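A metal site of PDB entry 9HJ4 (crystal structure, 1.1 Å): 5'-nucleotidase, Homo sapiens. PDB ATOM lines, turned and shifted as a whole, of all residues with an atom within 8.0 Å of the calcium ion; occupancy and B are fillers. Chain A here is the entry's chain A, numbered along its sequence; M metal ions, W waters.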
ATOM      1  N   VAL A 186      21.094  -5.048 -12.253  1.00  0.00           N
ATOM      2  CA  VAL A 186      22.192  -4.925 -11.314  1.00  0.00           C
ATOM      3  C   VAL A 186      23.347  -4.324 -12.108  1.00  0.00           C
ATOM      4  O   VAL A 186      23.935  -5.004 -12.942  1.00  0.00           O
ATOM      5  CB  VAL A 186      22.564  -6.280 -10.713  1.00  0.00           C
ATOM      6  CG1 VAL A 186      23.739  -6.123  -9.760  1.00  0.00           C
ATOM      7  CG2 VAL A 186      21.385  -6.874  -9.979  1.00  0.00           C
ATOM      8  N   ASN A 187      23.634  -3.041 -11.856  1.00  0.00           N
ATOM      9  CA  ASN A 187      24.574  -2.280 -12.663  1.00  0.00           C
ATOM     10  C   ASN A 187      25.930  -2.060 -11.999  1.00  0.00           C
ATOM     11  O   ASN A 187      26.771  -1.392 -12.597  1.00  0.00           O
ATOM     12  CB  ASN A 187      23.968  -0.937 -13.109  1.00  0.00           C
ATOM     13  CG  ASN A 187      23.598  -0.012 -11.951  1.00  0.00           C
ATOM     14  OD1 ASN A 187      24.197  -0.051 -10.881  1.00  0.00           O
ATOM     15  ND2 ASN A 187      22.614   0.852 -12.176  1.00  0.00           N
ATOM     16  N   LYS A 188      26.163  -2.606 -10.806  1.00  0.00           N
ATOM     17  CA  LYS A 188      27.440  -2.519 -10.119  1.00  0.00           C
ATOM     18  C   LYS A 188      27.868  -3.937  -9.805  1.00  0.00           C
ATOM     19  O   LYS A 188      27.172  -4.649  -9.075  1.00  0.00           O
ATOM     20  CB  LYS A 188      27.295  -1.696  -8.830  1.00  0.00           C
ATOM     21  CG  LYS A 188      27.034  -0.217  -9.134  1.00  0.00           C
ATOM     22  CD  LYS A 188      26.826   0.603  -7.876  1.00  0.00           C
ATOM     23  CE  LYS A 188      25.453   0.419  -7.277  1.00  0.00           C
ATOM     24  NZ  LYS A 188      24.384   1.033  -8.118  1.00  0.00           N
ATOM     25  N   ILE A 189      28.982  -4.364 -10.399  1.00  0.00           N
ATOM     26  CA  ILE A 189      29.375  -5.763 -10.410  1.00  0.00           C
ATOM     27  C   ILE A 189      30.830  -5.883  -9.998  1.00  0.00           C
ATOM     28  O   ILE A 189      31.719  -5.282 -10.614  1.00  0.00           O
ATOM     29  CB  ILE A 189      29.117  -6.418 -11.778  1.00  0.00           C
ATOM     30  CG1 ILE A 189      27.603  -6.393 -12.071  1.00  0.00           C
ATOM     31  CG2 ILE A 189      29.664  -7.834 -11.781  1.00  0.00           C
ATOM     32  CD1 ILE A 189      27.181  -7.024 -13.364  1.00  0.00           C
ATOM     33  N   ILE A 190      31.067  -6.675  -8.963  1.00  0.00           N
ATOM     34  CA  ILE A 190      32.402  -7.023  -8.502  1.00  0.00           C
ATOM     35  C   ILE A 190      32.664  -8.474  -8.883  1.00  0.00           C
ATOM     36  O   ILE A 190      31.853  -9.348  -8.557  1.00  0.00           O
ATOM     37  CB  ILE A 190      32.481  -6.907  -6.967  1.00  0.00           C
ATOM     38  CG1 ILE A 190      32.129  -5.510  -6.482  1.00  0.00           C
ATOM     39  CG2 ILE A 190      33.830  -7.394  -6.463  1.00  0.00           C
ATOM     40  CD1 ILE A 190      32.035  -5.417  -4.969  1.00  0.00           C
ATOM     41  N   GLY A 209      31.185  -5.681 -18.403  1.00  0.00           N
ATOM     42  CA  GLY A 209      30.302  -5.381 -17.305  1.00  0.00           C
ATOM     43  C   GLY A 209      30.907  -5.513 -15.920  1.00  0.00           C
ATOM     44  O   GLY A 209      30.266  -5.103 -14.960  1.00  0.00           O
ATOM     45  N   VAL A 210      32.103  -6.070 -15.786  1.00  0.00           N
ATOM     46  CA  VAL A 210      32.762  -6.127 -14.488  1.00  0.00           C
ATOM     47  C   VAL A 210      33.321  -4.746 -14.161  1.00  0.00           C
ATOM     48  O   VAL A 210      34.036  -4.138 -14.960  1.00  0.00           O
ATOM     49  CB  VAL A 210      33.880  -7.175 -14.516  1.00  0.00           C
ATOM     50  CG1 VAL A 210      34.775  -7.048 -13.286  1.00  0.00           C
ATOM     51  CG2 VAL A 210      33.292  -8.577 -14.590  1.00  0.00           C
ATOM     52  N   ASP A 211      32.998  -4.250 -12.964  1.00  0.00           N
ATOM     53  CA  ASP A 211      33.459  -2.922 -12.568  1.00  0.00           C
ATOM     54  C   ASP A 211      34.747  -2.930 -11.761  1.00  0.00           C
ATOM     55  O   ASP A 211      35.496  -1.944 -11.792  1.00  0.00           O
ATOM     56  CB  ASP A 211      32.366  -2.241 -11.753  1.00  0.00           C
ATOM     57  CG  ASP A 211      31.149  -1.916 -12.594  1.00  0.00           C
ATOM     58  OD1 ASP A 211      31.310  -1.345 -13.699  1.00  0.00           O
ATOM     59  OD2 ASP A 211      30.032  -2.262 -12.153  1.00  0.00           O
ATOM     60  N   VAL A 212      35.033  -3.998 -11.027  1.00  0.00           N
ATOM     61  CA  VAL A 212      36.228  -4.101 -10.204  1.00  0.00           C
ATOM     62  C   VAL A 212      36.469  -5.583  -9.956  1.00  0.00           C
ATOM     63  O   VAL A 212      35.516  -6.349  -9.757  1.00  0.00           O
ATOM     64  CB  VAL A 212      36.069  -3.333  -8.879  1.00  0.00           C
ATOM     65  CG1 VAL A 212      34.816  -3.789  -8.154  1.00  0.00           C
ATOM     66  CG2 VAL A 212      37.302  -3.517  -7.989  1.00  0.00           C
ATOM     67  N   ARG A 247      36.755   0.824 -20.829  1.00  0.00           N
ATOM     68  CA  ARG A 247      36.566   1.247 -19.459  1.00  0.00           C
ATOM     69  C   ARG A 247      37.853   1.019 -18.677  1.00  0.00           C
ATOM     70  O   ARG A 247      38.671   0.166 -19.027  1.00  0.00           O
ATOM     71  CB  ARG A 247      35.418   0.478 -18.775  1.00  0.00           C
ATOM     72  CG  ARG A 247      34.046   0.801 -19.362  1.00  0.00           C
ATOM     73  CD  ARG A 247      32.934  -0.037 -18.715  1.00  0.00           C
ATOM     74  NE  ARG A 247      33.212  -1.461 -18.807  1.00  0.00           N
ATOM     75  CZ  ARG A 247      33.460  -2.236 -17.751  1.00  0.00           C
ATOM     76  NH1 ARG A 247      33.356  -1.790 -16.516  1.00  0.00           N
ATOM     77  NH2 ARG A 247      33.814  -3.504 -17.950  1.00  0.00           N
ATOM     78  N   PHE A 268      30.856   5.559  -7.866  1.00  0.00           N
ATOM     79  CA  PHE A 268      30.012   5.138  -8.969  1.00  0.00           C
ATOM     80  C   PHE A 268      29.061   6.268  -9.334  1.00  0.00           C
ATOM     81  O   PHE A 268      28.595   7.017  -8.469  1.00  0.00           O
ATOM     82  CB  PHE A 268      29.127   3.955  -8.574  1.00  0.00           C
ATOM     83  CG  PHE A 268      29.845   2.663  -8.396  1.00  0.00           C
ATOM     84  CD1 PHE A 268      30.055   1.817  -9.470  1.00  0.00           C
ATOM     85  CD2 PHE A 268      30.244   2.248  -7.134  1.00  0.00           C
ATOM     86  CE1 PHE A 268      30.677   0.587  -9.298  1.00  0.00           C
ATOM     87  CE2 PHE A 268      30.872   1.026  -6.972  1.00  0.00           C
ATOM     88  CZ  PHE A 268      31.076   0.197  -8.055  1.00  0.00           C
ATOM     89  N   ASP A 269      28.739   6.356 -10.625  1.00  0.00           N
ATOM     90  CA  ASP A 269      27.621   7.195 -11.046  1.00  0.00           C
ATOM     91  C   ASP A 269      26.319   6.407 -10.935  1.00  0.00           C
ATOM     92  O   ASP A 269      26.286   5.221 -10.578  1.00  0.00           O
ATOM     93  CB  ASP A 269      27.867   7.829 -12.426  1.00  0.00           C
ATOM     94  CG  ASP A 269      27.764   6.841 -13.586  1.00  0.00           C
ATOM     95  OD1 ASP A 269      27.280   5.710 -13.416  1.00  0.00           O
ATOM     96  OD2 ASP A 269      28.158   7.227 -14.709  1.00  0.00           O
ATOM     97  N   ARG A 271      24.409   5.185 -13.087  1.00  0.00           N
ATOM     98  CA  ARG A 271      24.294   4.068 -14.005  1.00  0.00           C
ATOM     99  C   ARG A 271      25.245   2.927 -13.659  1.00  0.00           C
ATOM    100  O   ARG A 271      25.321   1.948 -14.404  1.00  0.00           O
ATOM    101  CB  ARG A 271      24.557   4.508 -15.440  1.00  0.00           C
ATOM    102  CG  ARG A 271      23.431   5.365 -16.034  1.00  0.00           C
ATOM    103  CD  ARG A 271      23.722   5.760 -17.479  1.00  0.00           C
ATOM    104  N   GLY A 272      25.959   3.035 -12.547  1.00  0.00           N
ATOM    105  CA  GLY A 272      26.860   1.978 -12.127  1.00  0.00           C
ATOM    106  C   GLY A 272      28.233   1.996 -12.766  1.00  0.00           C
ATOM    107  O   GLY A 272      28.958   1.005 -12.655  1.00  0.00           O
ATOM    108  N   ASN A 273      28.608   3.082 -13.433  1.00  0.00           N
ATOM    109  CA  ASN A 273      29.955   3.193 -13.976  1.00  0.00           C
ATOM    110  C   ASN A 273      30.903   3.735 -12.913  1.00  0.00           C
ATOM    111  O   ASN A 273      30.553   4.634 -12.145  1.00  0.00           O
ATOM    112  CB  ASN A 273      29.963   4.133 -15.166  1.00  0.00           C
ATOM    113  CG  ASN A 273      29.069   3.656 -16.254  1.00  0.00           C
ATOM    114  OD1 ASN A 273      29.224   2.541 -16.760  1.00  0.00           O
ATOM    115  ND2 ASN A 273      28.067   4.462 -16.591  1.00  0.00           N
ATOM    116  N   VAL A 274      32.120   3.172 -12.883  1.00  0.00           N
ATOM    117  CA  VAL A 274      33.142   3.662 -11.973  1.00  0.00           C
ATOM    118  C   VAL A 274      33.671   4.994 -12.487  1.00  0.00           C
ATOM    119  O   VAL A 274      34.199   5.083 -13.599  1.00  0.00           O
ATOM    120  CB  VAL A 274      34.276   2.632 -11.830  1.00  0.00           C
ATOM    121  CG1 VAL A 274      35.401   3.206 -11.001  1.00  0.00           C
ATOM    122  CG2 VAL A 274      33.739   1.336 -11.229  1.00  0.00           C
HETATM  123 CA    CA M   1      28.695  -1.085 -13.782  1.00  0.00          CA
HETATM  124  O   HOH W   1      30.139  -0.207 -16.370  1.00  0.00           O
HETATM  125  O   HOH W   2      27.219  -0.006 -15.354  1.00  0.00           O
HETATM  126  O   HOH W   3      28.344  -3.200 -14.964  1.00  0.00           O
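The backbone NH of Gly 272 lies within hydrogen-bond range of the side-chain carboxylate of Asp 269, at 3.1 Å.
The side-chain amino group of Lys 188 is in hydrogen-bond range of the side-chain amide oxygen of Asn 187 (3.0 Å).
The backbone carbonyl oxygen (O) of Ile 189 is in hydrogen-bond range of the backbone NH (N) of Asp 211, 2.9 Å away.
The side-chain carboxylate (OD1) of Asp 211 sits close to the guanidinium group (NH1) of Arg 247 (3.5 Å).
Within 4 Å of the calcium ion: Asn 187, Asp 211 and Gly 272.
The calcium ion is bound by the backbone carbonyl oxygen (O) of Asn 187 (2.3 Å), the backbone carbonyl oxygen (O) of Gly 272 (2.4 Å), water W2 (2.4 Å), the side-chain carboxylate (OD2) of Asp 211 (2.4 Å), water W3 (2.4 Å) and the side-chain carboxylate (OD1) of Asp 211 (2.6 Å).
The calcium ion has six donor atoms within binding distance.
Slightly farther from the calcium ion lies water W1 (3.1 Å).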
